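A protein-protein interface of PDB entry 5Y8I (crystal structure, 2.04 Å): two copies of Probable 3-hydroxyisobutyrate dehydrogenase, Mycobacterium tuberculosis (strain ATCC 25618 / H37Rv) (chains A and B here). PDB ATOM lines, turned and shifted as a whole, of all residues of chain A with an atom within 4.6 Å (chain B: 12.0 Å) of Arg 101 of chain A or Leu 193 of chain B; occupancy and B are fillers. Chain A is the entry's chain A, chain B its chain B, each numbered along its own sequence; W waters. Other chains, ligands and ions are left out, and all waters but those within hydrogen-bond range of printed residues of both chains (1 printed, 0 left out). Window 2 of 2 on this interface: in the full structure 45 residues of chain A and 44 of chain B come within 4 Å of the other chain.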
ATOM      1  N   VAL A  97      -7.899 -19.658 -13.778  1.00  0.00           N
ATOM      2  CA  VAL A  97      -7.083 -20.299 -14.784  1.00  0.00           C
ATOM      3  C   VAL A  97      -7.679 -21.668 -15.139  1.00  0.00           C
ATOM      4  O   VAL A  97      -7.779 -21.984 -16.265  1.00  0.00           O
ATOM      5  CB  VAL A  97      -5.606 -20.426 -14.357  1.00  0.00           C
ATOM      6  CG1 VAL A  97      -4.773 -21.112 -15.410  1.00  0.00           C
ATOM      7  CG2 VAL A  97      -5.028 -19.084 -14.029  1.00  0.00           C
ATOM      8  N   THR A  98      -8.043 -22.443 -14.129  1.00  0.00           N
ATOM      9  CA  THR A  98      -8.661 -23.747 -14.298  1.00  0.00           C
ATOM     10  C   THR A  98      -9.943 -23.649 -15.111  1.00  0.00           C
ATOM     11  O   THR A  98     -10.110 -24.362 -16.037  1.00  0.00           O
ATOM     12  CB  THR A  98      -8.979 -24.433 -12.959  1.00  0.00           C
ATOM     13  OG1 THR A  98      -7.828 -24.447 -12.156  1.00  0.00           O
ATOM     14  CG2 THR A  98      -9.412 -25.844 -13.172  1.00  0.00           C
ATOM     15  N   ASP A  99     -10.834 -22.762 -14.700  1.00  0.00           N
ATOM     16  CA  ASP A  99     -12.094 -22.530 -15.427  1.00  0.00           C
ATOM     17  C   ASP A  99     -11.845 -22.066 -16.866  1.00  0.00           C
ATOM     18  O   ASP A  99     -12.509 -22.528 -17.776  1.00  0.00           O
ATOM     19  CB  ASP A  99     -12.991 -21.519 -14.694  1.00  0.00           C
ATOM     20  CG  ASP A  99     -13.608 -22.090 -13.410  1.00  0.00           C
ATOM     21  OD1 ASP A  99     -13.551 -23.316 -13.175  1.00  0.00           O
ATOM     22  OD2 ASP A  99     -14.182 -21.308 -12.630  1.00  0.00           O
ATOM     23  N   ALA A 100     -10.873 -21.182 -17.064  1.00  0.00           N
ATOM     24  CA  ALA A 100     -10.528 -20.720 -18.399  1.00  0.00           C
ATOM     25  C   ALA A 100     -10.108 -21.871 -19.296  1.00  0.00           C
ATOM     26  O   ALA A 100     -10.584 -21.986 -20.426  1.00  0.00           O
ATOM     27  CB  ALA A 100      -9.427 -19.671 -18.338  1.00  0.00           C
ATOM     28  N   ARG A 101      -9.241 -22.737 -18.780  1.00  0.00           N
ATOM     29  CA  ARG A 101      -8.770 -23.884 -19.556  1.00  0.00           C
ATOM     30  C   ARG A 101      -9.854 -24.921 -19.840  1.00  0.00           C
ATOM     31  O   ARG A 101      -9.896 -25.481 -20.933  1.00  0.00           O
ATOM     32  CB  ARG A 101      -7.546 -24.523 -18.903  1.00  0.00           C
ATOM     33  CG  ARG A 101      -6.310 -23.629 -19.011  1.00  0.00           C
ATOM     34  CD  ARG A 101      -5.132 -24.129 -18.177  1.00  0.00           C
ATOM     35  NE  ARG A 101      -3.946 -23.329 -18.458  1.00  0.00           N
ATOM     36  CZ  ARG A 101      -2.864 -23.214 -17.681  1.00  0.00           C
ATOM     37  NH1 ARG A 101      -2.770 -23.834 -16.506  1.00  0.00           N
ATOM     38  NH2 ARG A 101      -1.863 -22.430 -18.084  1.00  0.00           N
ATOM     39  N   GLU A 102     -10.741 -25.158 -18.886  1.00  0.00           N
ATOM     40  CA  GLU A 102     -11.859 -26.089 -19.103  1.00  0.00           C
ATOM     41  C   GLU A 102     -12.770 -25.576 -20.224  1.00  0.00           C
ATOM     42  O   GLU A 102     -13.131 -26.291 -21.151  1.00  0.00           O
ATOM     43  CB  GLU A 102     -12.661 -26.231 -17.819  1.00  0.00           C
ATOM     44  CG  GLU A 102     -13.776 -27.263 -17.868  1.00  0.00           C
ATOM     45  CD  GLU A 102     -14.593 -27.302 -16.586  1.00  0.00           C
ATOM     46  OE1 GLU A 102     -15.653 -27.967 -16.577  1.00  0.00           O
ATOM     47  OE2 GLU A 102     -14.186 -26.664 -15.587  1.00  0.00           O
ATOM     48  N   VAL A 103     -13.146 -24.309 -20.151  1.00  0.00           N
ATOM     49  CA  VAL A 103     -13.995 -23.740 -21.179  1.00  0.00           C
ATOM     50  C   VAL A 103     -13.325 -23.624 -22.559  1.00  0.00           C
ATOM     51  O   VAL A 103     -13.980 -23.702 -23.532  1.00  0.00           O
ATOM     52  CB  VAL A 103     -14.720 -22.441 -20.795  1.00  0.00           C
ATOM     53  CG1 VAL A 103     -15.517 -22.551 -19.516  1.00  0.00           C
ATOM     54  CG2 VAL A 103     -13.811 -21.264 -20.863  1.00  0.00           C
ATOM     55  N   HIS A 104     -12.019 -23.418 -22.590  1.00  0.00           N
ATOM     56  CA  HIS A 104     -11.289 -23.397 -23.824  1.00  0.00           C
ATOM     57  C   HIS A 104     -11.367 -24.786 -24.476  1.00  0.00           C
ATOM     58  O   HIS A 104     -11.668 -24.901 -25.621  1.00  0.00           O
ATOM     59  CB  HIS A 104      -9.836 -22.989 -23.589  1.00  0.00           C
ATOM     60  CG  HIS A 104      -8.951 -23.195 -24.772  1.00  0.00           C
ATOM     61  ND1 HIS A 104      -8.812 -22.265 -25.763  1.00  0.00           N
ATOM     62  CD2 HIS A 104      -8.192 -24.241 -25.135  1.00  0.00           C
ATOM     63  CE1 HIS A 104      -7.997 -22.725 -26.678  1.00  0.00           C
ATOM     64  NE2 HIS A 104      -7.616 -23.926 -26.325  1.00  0.00           N
ATOM     65  N   ALA A 105     -11.082 -25.807 -23.695  1.00  0.00           N
ATOM     66  CA  ALA A 105     -11.145 -27.188 -24.166  1.00  0.00           C
ATOM     67  C   ALA A 105     -12.563 -27.581 -24.635  1.00  0.00           C
ATOM     68  O   ALA A 105     -12.728 -28.254 -25.657  1.00  0.00           O
ATOM     69  CB  ALA A 105     -10.646 -28.151 -23.083  1.00  0.00           C
ATOM     70  N   ALA A 162      -3.754 -21.261 -23.760  1.00  0.00           N
ATOM     71  CA  ALA A 162      -5.006 -21.102 -23.031  1.00  0.00           C
ATOM     72  C   ALA A 162      -4.800 -21.068 -21.512  1.00  0.00           C
ATOM     73  O   ALA A 162      -4.093 -21.901 -20.956  1.00  0.00           O
ATOM     74  CB  ALA A 162      -5.961 -22.230 -23.393  1.00  0.00           C
ATOM     75  N   GLY A 163      -5.429 -20.097 -20.863  1.00  0.00           N
ATOM     76  CA  GLY A 163      -5.252 -19.820 -19.435  1.00  0.00           C
ATOM     77  C   GLY A 163      -4.191 -18.776 -19.088  1.00  0.00           C
ATOM     78  O   GLY A 163      -4.266 -18.149 -18.028  1.00  0.00           O
ATOM     79  N   ALA A 164      -3.209 -18.573 -19.970  1.00  0.00           N
ATOM     80  CA  ALA A 164      -2.102 -17.637 -19.713  1.00  0.00           C
ATOM     81  C   ALA A 164      -2.538 -16.181 -19.527  1.00  0.00           C
ATOM     82  O   ALA A 164      -1.890 -15.438 -18.787  1.00  0.00           O
ATOM     83  CB  ALA A 164      -1.063 -17.735 -20.819  1.00  0.00           C
ATOM     84  N   ALA A 167      -3.887 -16.076 -16.002  1.00  0.00           N
ATOM     85  CA  ALA A 167      -2.726 -16.202 -15.114  1.00  0.00           C
ATOM     86  C   ALA A 167      -1.919 -14.914 -15.022  1.00  0.00           C
ATOM     87  O   ALA A 167      -1.492 -14.534 -13.935  1.00  0.00           O
ATOM     88  CB  ALA A 167      -1.811 -17.332 -15.581  1.00  0.00           C
ATOM     89  N   ALA A 252      -5.909 -19.801  -7.447  1.00  0.00           N
ATOM     90  CA  ALA A 252      -4.729 -20.250  -8.170  1.00  0.00           C
ATOM     91  C   ALA A 252      -3.656 -20.828  -7.220  1.00  0.00           C
ATOM     92  O   ALA A 252      -3.039 -21.861  -7.523  1.00  0.00           O
ATOM     93  CB  ALA A 252      -4.161 -19.115  -8.992  1.00  0.00           C
ATOM     94  N   THR A 256      -2.506 -24.823  -7.117  1.00  0.00           N
ATOM     95  CA  THR A 256      -1.123 -25.183  -7.454  1.00  0.00           C
ATOM     96  C   THR A 256      -0.301 -25.629  -6.245  1.00  0.00           C
ATOM     97  O   THR A 256       0.759 -26.196  -6.410  1.00  0.00           O
ATOM     98  CB  THR A 256      -0.374 -24.007  -8.105  1.00  0.00           C
ATOM     99  OG1 THR A 256      -0.453 -22.849  -7.261  1.00  0.00           O
ATOM    100  CG2 THR A 256      -0.979 -23.691  -9.461  1.00  0.00           C
ATOM    101  N   ALA B 182       7.099 -10.115  -3.259  1.00  0.00           N
ATOM    102  CA  ALA B 182       5.875 -10.224  -4.060  1.00  0.00           C
ATOM    103  C   ALA B 182       6.167 -10.607  -5.514  1.00  0.00           C
ATOM    104  O   ALA B 182       5.431 -11.410  -6.097  1.00  0.00           O
ATOM    105  CB  ALA B 182       5.060  -8.939  -4.005  1.00  0.00           C
ATOM    106  N   ILE B 183       7.240 -10.048  -6.079  1.00  0.00           N
ATOM    107  CA  ILE B 183       7.662 -10.388  -7.435  1.00  0.00           C
ATOM    108  C   ILE B 183       8.107 -11.852  -7.489  1.00  0.00           C
ATOM    109  O   ILE B 183       7.733 -12.560  -8.413  1.00  0.00           O
ATOM    110  CB  ILE B 183       8.741  -9.416  -7.970  1.00  0.00           C
ATOM    111  CG1 ILE B 183       8.112  -8.041  -8.272  1.00  0.00           C
ATOM    112  CG2 ILE B 183       9.471  -9.972  -9.193  1.00  0.00           C
ATOM    113  CD1 ILE B 183       7.065  -8.010  -9.369  1.00  0.00           C
ATOM    114  N   ALA B 184       8.869 -12.302  -6.490  1.00  0.00           N
ATOM    115  CA  ALA B 184       9.259 -13.698  -6.409  1.00  0.00           C
ATOM    116  C   ALA B 184       8.041 -14.648  -6.377  1.00  0.00           C
ATOM    117  O   ALA B 184       8.026 -15.635  -7.111  1.00  0.00           O
ATOM    118  CB  ALA B 184      10.173 -13.936  -5.218  1.00  0.00           C
ATOM    119  N   GLU B 185       7.034 -14.322  -5.559  1.00  0.00           N
ATOM    120  CA  GLU B 185       5.789 -15.086  -5.461  1.00  0.00           C
ATOM    121  C   GLU B 185       5.064 -15.199  -6.805  1.00  0.00           C
ATOM    122  O   GLU B 185       4.606 -16.292  -7.189  1.00  0.00           O
ATOM    123  CB  GLU B 185       4.825 -14.456  -4.437  1.00  0.00           C
ATOM    124  CG  GLU B 185       5.285 -14.511  -2.984  1.00  0.00           C
ATOM    125  CD  GLU B 185       4.360 -13.752  -2.024  1.00  0.00           C
ATOM    126  OE1 GLU B 185       3.254 -13.280  -2.419  1.00  0.00           O
ATOM    127  OE2 GLU B 185       4.734 -13.640  -0.833  1.00  0.00           O
ATOM    128  N   ALA B 186       4.967 -14.067  -7.507  1.00  0.00           N
ATOM    129  CA  ALA B 186       4.330 -14.009  -8.815  1.00  0.00           C
ATOM    130  C   ALA B 186       5.004 -14.936  -9.809  1.00  0.00           C
ATOM    131  O   ALA B 186       4.322 -15.673 -10.515  1.00  0.00           O
ATOM    132  CB  ALA B 186       4.339 -12.587  -9.349  1.00  0.00           C
ATOM    133  N   PHE B 187       6.340 -14.893  -9.860  1.00  0.00           N
ATOM    134  CA  PHE B 187       7.095 -15.704 -10.805  1.00  0.00           C
ATOM    135  C   PHE B 187       6.975 -17.197 -10.527  1.00  0.00           C
ATOM    136  O   PHE B 187       6.926 -17.979 -11.462  1.00  0.00           O
ATOM    137  CB  PHE B 187       8.575 -15.278 -10.877  1.00  0.00           C
ATOM    138  CG  PHE B 187       8.824 -14.161 -11.840  1.00  0.00           C
ATOM    139  CD1 PHE B 187       8.893 -14.418 -13.206  1.00  0.00           C
ATOM    140  CD2 PHE B 187       8.962 -12.861 -11.405  1.00  0.00           C
ATOM    141  CE1 PHE B 187       9.098 -13.398 -14.114  1.00  0.00           C
ATOM    142  CE2 PHE B 187       9.172 -11.829 -12.307  1.00  0.00           C
ATOM    143  CZ  PHE B 187       9.240 -12.101 -13.667  1.00  0.00           C
ATOM    144  N   VAL B 188       6.908 -17.587  -9.260  1.00  0.00           N
ATOM    145  CA  VAL B 188       6.796 -18.991  -8.908  1.00  0.00           C
ATOM    146  C   VAL B 188       5.376 -19.471  -9.192  1.00  0.00           C
ATOM    147  O   VAL B 188       5.197 -20.539  -9.755  1.00  0.00           O
ATOM    148  CB  VAL B 188       7.176 -19.241  -7.436  1.00  0.00           C
ATOM    149  CG1 VAL B 188       6.958 -20.703  -7.063  1.00  0.00           C
ATOM    150  CG2 VAL B 188       8.644 -18.886  -7.211  1.00  0.00           C
ATOM    151  N   LEU B 189       4.380 -18.674  -8.806  1.00  0.00           N
ATOM    152  CA  LEU B 189       2.973 -18.964  -9.107  1.00  0.00           C
ATOM    153  C   LEU B 189       2.759 -19.108 -10.615  1.00  0.00           C
ATOM    154  O   LEU B 189       2.122 -20.053 -11.057  1.00  0.00           O
ATOM    155  CB  LEU B 189       2.058 -17.869  -8.548  1.00  0.00           C
ATOM    156  CG  LEU B 189       0.551 -18.032  -8.827  1.00  0.00           C
ATOM    157  CD1 LEU B 189       0.002 -19.352  -8.291  1.00  0.00           C
ATOM    158  CD2 LEU B 189      -0.202 -16.867  -8.219  1.00  0.00           C
ATOM    159  N   ALA B 190       3.307 -18.174 -11.386  1.00  0.00           N
ATOM    160  CA  ALA B 190       3.283 -18.238 -12.841  1.00  0.00           C
ATOM    161  C   ALA B 190       3.846 -19.559 -13.351  1.00  0.00           C
ATOM    162  O   ALA B 190       3.245 -20.169 -14.231  1.00  0.00           O
ATOM    163  CB  ALA B 190       4.056 -17.080 -13.447  1.00  0.00           C
ATOM    164  N   GLU B 191       4.980 -20.004 -12.803  1.00  0.00           N
ATOM    165  CA  GLU B 191       5.566 -21.278 -13.231  1.00  0.00           C
ATOM    166  C   GLU B 191       4.641 -22.444 -12.917  1.00  0.00           C
ATOM    167  O   GLU B 191       4.465 -23.314 -13.760  1.00  0.00           O
ATOM    168  CB  GLU B 191       6.965 -21.529 -12.646  1.00  0.00           C
ATOM    169  CG  GLU B 191       7.660 -22.813 -13.152  1.00  0.00           C
ATOM    170  CD  GLU B 191       7.875 -22.886 -14.685  1.00  0.00           C
ATOM    171  OE1 GLU B 191       6.890 -23.067 -15.455  1.00  0.00           O
ATOM    172  OE2 GLU B 191       9.050 -22.809 -15.141  1.00  0.00           O
ATOM    173  N   LYS B 192       4.030 -22.457 -11.735  1.00  0.00           N
ATOM    174  CA  LYS B 192       3.079 -23.526 -11.401  1.00  0.00           C
ATOM    175  C   LYS B 192       1.811 -23.488 -12.266  1.00  0.00           C
ATOM    176  O   LYS B 192       1.178 -24.508 -12.461  1.00  0.00           O
ATOM    177  CB  LYS B 192       2.698 -23.518  -9.916  1.00  0.00           C
ATOM    178  CG  LYS B 192       3.857 -23.752  -8.939  1.00  0.00           C
ATOM    179  CD  LYS B 192       3.346 -24.162  -7.569  1.00  0.00           C
ATOM    180  CE  LYS B 192       4.345 -23.942  -6.442  1.00  0.00           C
ATOM    181  NZ  LYS B 192       5.723 -24.397  -6.723  1.00  0.00           N
ATOM    182  N   LEU B 193       1.445 -22.313 -12.764  1.00  0.00           N
ATOM    183  CA  LEU B 193       0.298 -22.148 -13.661  1.00  0.00           C
ATOM    184  C   LEU B 193       0.610 -22.389 -15.139  1.00  0.00           C
ATOM    185  O   LEU B 193      -0.297 -22.344 -15.953  1.00  0.00           O
ATOM    186  CB  LEU B 193      -0.321 -20.742 -13.497  1.00  0.00           C
ATOM    187  CG  LEU B 193      -1.015 -20.468 -12.164  1.00  0.00           C
ATOM    188  CD1 LEU B 193      -1.378 -18.993 -12.056  1.00  0.00           C
ATOM    189  CD2 LEU B 193      -2.248 -21.345 -11.969  1.00  0.00           C
ATOM    190  N   GLY B 194       1.869 -22.647 -15.480  1.00  0.00           N
ATOM    191  CA  GLY B 194       2.296 -22.796 -16.873  1.00  0.00           C
ATOM    192  C   GLY B 194       2.493 -21.495 -17.647  1.00  0.00           C
ATOM    193  O   GLY B 194       2.570 -21.519 -18.870  1.00  0.00           O
ATOM    194  N   LEU B 195       2.583 -20.364 -16.948  1.00  0.00           N
ATOM    195  CA  LEU B 195       2.859 -19.077 -17.579  1.00  0.00           C
ATOM    196  C   LEU B 195       4.380 -18.884 -17.594  1.00  0.00           C
ATOM    197  O   LEU B 195       5.002 -18.957 -16.543  1.00  0.00           O
ATOM    198  CB  LEU B 195       2.167 -17.963 -16.790  1.00  0.00           C
ATOM    199  CG  LEU B 195       2.420 -16.516 -17.199  1.00  0.00           C
ATOM    200  CD1 LEU B 195       1.907 -16.276 -18.606  1.00  0.00           C
ATOM    201  CD2 LEU B 195       1.758 -15.577 -16.207  1.00  0.00           C
ATOM    202  N   SER B 196       4.983 -18.666 -18.769  1.00  0.00           N
ATOM    203  CA  SER B 196       6.457 -18.550 -18.859  1.00  0.00           C
ATOM    204  C   SER B 196       6.983 -17.300 -18.149  1.00  0.00           C
ATOM    205  O   SER B 196       6.275 -16.301 -18.025  1.00  0.00           O
ATOM    206  CB  SER B 196       6.956 -18.544 -20.311  1.00  0.00           C
ATOM    207  OG  SER B 196       6.743 -17.279 -20.912  1.00  0.00           O
ATOM    208  N   ALA B 197       8.236 -17.376 -17.705  1.00  0.00           N
ATOM    209  CA  ALA B 197       8.873 -16.274 -17.004  1.00  0.00           C
ATOM    210  C   ALA B 197       8.944 -15.054 -17.892  1.00  0.00           C
ATOM    211  O   ALA B 197       8.630 -13.948 -17.453  1.00  0.00           O
ATOM    212  CB  ALA B 197      10.263 -16.662 -16.527  1.00  0.00           C
ATOM    213  N   GLN B 198       9.330 -15.257 -19.150  1.00  0.00           N
ATOM    214  CA  GLN B 198       9.381 -14.157 -20.103  1.00  0.00           C
ATOM    215  C   GLN B 198       8.026 -13.478 -20.263  1.00  0.00           C
ATOM    216  O   GLN B 198       7.955 -12.245 -20.317  1.00  0.00           O
ATOM    217  CB  GLN B 198       9.894 -14.649 -21.460  1.00  0.00           C
ATOM    218  CG  GLN B 198      10.212 -13.540 -22.453  1.00  0.00           C
ATOM    219  CD  GLN B 198      11.294 -12.610 -21.935  1.00  0.00           C
ATOM    220  OE1 GLN B 198      12.358 -13.065 -21.552  1.00  0.00           O
ATOM    221  NE2 GLN B 198      11.005 -11.317 -21.876  1.00  0.00           N
ATOM    222  N   SER B 199       6.953 -14.273 -20.330  1.00  0.00           N
ATOM    223  CA  SER B 199       5.603 -13.720 -20.512  1.00  0.00           C
ATOM    224  C   SER B 199       5.162 -12.906 -19.313  1.00  0.00           C
ATOM    225  O   SER B 199       4.687 -11.782 -19.479  1.00  0.00           O
ATOM    226  CB  SER B 199       4.564 -14.811 -20.766  1.00  0.00           C
ATOM    227  OG  SER B 199       4.906 -15.563 -21.911  1.00  0.00           O
ATOM    228  N   LEU B 200       5.344 -13.452 -18.111  1.00  0.00           N
ATOM    229  CA  LEU B 200       5.018 -12.710 -16.905  1.00  0.00           C
ATOM    230  C   LEU B 200       5.822 -11.413 -16.841  1.00  0.00           C
ATOM    231  O   LEU B 200       5.259 -10.362 -16.558  1.00  0.00           O
ATOM    232  CB  LEU B 200       5.233 -13.537 -15.637  1.00  0.00           C
ATOM    233  CG  LEU B 200       4.815 -12.764 -14.371  1.00  0.00           C
ATOM    234  CD1 LEU B 200       3.303 -12.591 -14.325  1.00  0.00           C
ATOM    235  CD2 LEU B 200       5.331 -13.426 -13.097  1.00  0.00           C
ATOM    236  N   VAL B 203       4.413  -8.820 -19.200  1.00  0.00           N
ATOM    237  CA  VAL B 203       3.130  -8.297 -18.719  1.00  0.00           C
ATOM    238  C   VAL B 203       3.301  -7.340 -17.537  1.00  0.00           C
ATOM    239  O   VAL B 203       2.823  -6.204 -17.598  1.00  0.00           O
ATOM    240  CB  VAL B 203       2.142  -9.421 -18.358  1.00  0.00           C
ATOM    241  CG1 VAL B 203       0.890  -8.853 -17.700  1.00  0.00           C
ATOM    242  CG2 VAL B 203       1.748 -10.169 -19.607  1.00  0.00           C
ATOM    243  N   ILE B 204       3.968  -7.794 -16.475  1.00  0.00           N
ATOM    244  CA  ILE B 204       4.112  -6.980 -15.271  1.00  0.00           C
ATOM    245  C   ILE B 204       4.851  -5.690 -15.592  1.00  0.00           C
ATOM    246  O   ILE B 204       4.420  -4.624 -15.139  1.00  0.00           O
ATOM    247  CB  ILE B 204       4.790  -7.720 -14.084  1.00  0.00           C
ATOM    248  CG1 ILE B 204       3.891  -8.853 -13.582  1.00  0.00           C
ATOM    249  CG2 ILE B 204       5.016  -6.767 -12.906  1.00  0.00           C
ATOM    250  CD1 ILE B 204       4.327  -9.490 -12.261  1.00  0.00           C
ATOM    251  N   LEU B 289      10.275 -20.073  -1.754  1.00  0.00           N
ATOM    252  CA  LEU B 289       8.920 -20.298  -2.280  1.00  0.00           C
ATOM    253  C   LEU B 289       8.806 -21.511  -3.199  1.00  0.00           C
ATOM    254  O   LEU B 289       7.701 -21.846  -3.638  1.00  0.00           O
ATOM    255  CB  LEU B 289       8.457 -19.059  -3.046  1.00  0.00           C
ATOM    256  CG  LEU B 289       8.691 -17.700  -2.371  1.00  0.00           C
ATOM    257  CD1 LEU B 289       8.361 -16.565  -3.324  1.00  0.00           C
ATOM    258  CD2 LEU B 289       7.879 -17.588  -1.090  1.00  0.00           C
ATOM    259  N   ARG B 290       9.935 -22.134  -3.484  1.00  0.00           N
ATOM    260  CA  ARG B 290      10.019 -23.319  -4.305  1.00  0.00           C
ATOM    261  C   ARG B 290      10.346 -24.537  -3.472  1.00  0.00           C
ATOM    262  O   ARG B 290      11.107 -24.478  -2.548  1.00  0.00           O
ATOM    263  CB  ARG B 290      11.108 -23.195  -5.359  1.00  0.00           C
ATOM    264  CG  ARG B 290      10.981 -22.068  -6.342  1.00  0.00           C
ATOM    265  CD  ARG B 290      11.592 -22.452  -7.654  1.00  0.00           C
ATOM    266  NE  ARG B 290      11.443 -21.481  -8.713  1.00  0.00           N
ATOM    267  CZ  ARG B 290      12.309 -20.525  -8.950  1.00  0.00           C
ATOM    268  NH1 ARG B 290      13.367 -20.415  -8.186  1.00  0.00           N
ATOM    269  NH2 ARG B 290      12.108 -19.697  -9.942  1.00  0.00           N
HETATM  270  O   HOH W   1      -0.777 -25.291 -14.320  1.00  0.00           O
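The guanidinium group (NH2) of Arg 101 of chain A lies within hydrogen-bond range of the backbone carbonyl oxygen (O) of Leu 193 of chain B (2.6 Å).
The guanidinium group (NE) of Arg 101 of chain A is in hydrogen-bond range of the backbone carbonyl oxygen (O) of Ala 162 of chain A, 2.9 Å away. The backbone carbonyl oxygen (O) of Ala 252 of chain A lies within hydrogen-bond range of the side-chain hydroxyl (OG1) of Thr 256 of chain A (2.8 Å). The backbone carbonyl oxygen of Ala 190 of chain B sits at hydrogen-bond distance from the backbone NH of Leu 195 of chain B, 2.8 Å away.
Ala 164 of chain A touches Leu 195 of chain B (O to CD1, 3.9 Å). Leu 193 of chain B touches Ala 167 of chain A (CD1 to CB, 3.9 Å). Leu 195 of chain B touches Ala 167 of chain A (CD2 to C, 3.9 Å). OG1 of Thr 256 of chain A touches CD1 of Leu 189 of chain B, at 3.7 Å. O of Thr 256 of chain A touches CD of Lys 192 of chain B, 3.5 Å away. CG2 of Thr 256 of chain A touches CD2 of Leu 193 of chain B (3.7 Å).
No residue of chain B comes within 4 Å of Val 97 of chain A. No residue of chain B comes within 4 Å of Thr 98 of chain A. No residue of chain B comes within 4 Å of Ala 100 of chain A. Arg 101 of chain A touches one residue of chain B. No residue of chain B comes within 4 Å of Glu 102 of chain A. No residue of chain B comes within 4 Å of Val 103 of chain A. No residue of chain B comes within 4 Å of His 104 of chain A. Ala 105 of chain A touches none of the printed residues of chain B. No residue of chain B comes within 4 Å of Ala 162 of chain A. No residue of chain B comes within 4 Å of Gly 163 of chain A. Printed residues of chain A within 4 Å of Leu 189 of chain B: Thr 256 (3.7 Å). Of the printed residues of chain A, Lys 192 of chain B touches Thr 256. Of chain A, only Arg 101, Ala 167 and Thr 256 come within 4 Å of Leu 193 of chain B. Of the printed residues of chain A, Leu 195 of chain B touches Ala 164 (3.9 Å) and Ala 167 (3.9 Å). Leu 289 of chain B touches none of the printed residues of chain A. Arg 290 of chain B touches none of the printed residues of chain A. The nearest printed residue of chain A that does not touch Leu 193 of chain B is Val 97 of chain A (4.1 Å).
Of the 15 printed residues of chain A, 4 touch a printed residue of chain B. Hydrophobic or aromatic side chains of chain A within 4 Å of the printed part of chain B: Ala 164 and Ala 167. Of the 23 printed residues of chain B, 4 touch a printed residue of chain A. Printed residues of chain B that touch a printed residue of chain A: Leu 189, Lys 192, Leu 193 and Leu 195. Among the printed residues, no Asp or Glu carboxylate lies within 4 Å of a Lys or Arg side-chain nitrogen of the other chain.
No position is printed for both chains. Of the 7 pairs that touch across the chains among the printed residues, none has its exchanged pair printed and touching as well.
Water W1 lies within hydrogen-bond range of O of Lys 192 of chain B (2.8 Å), NH1 of Arg 101 of chain A (3.3 Å) and O of Leu 193 of chain B (3.4 Å).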
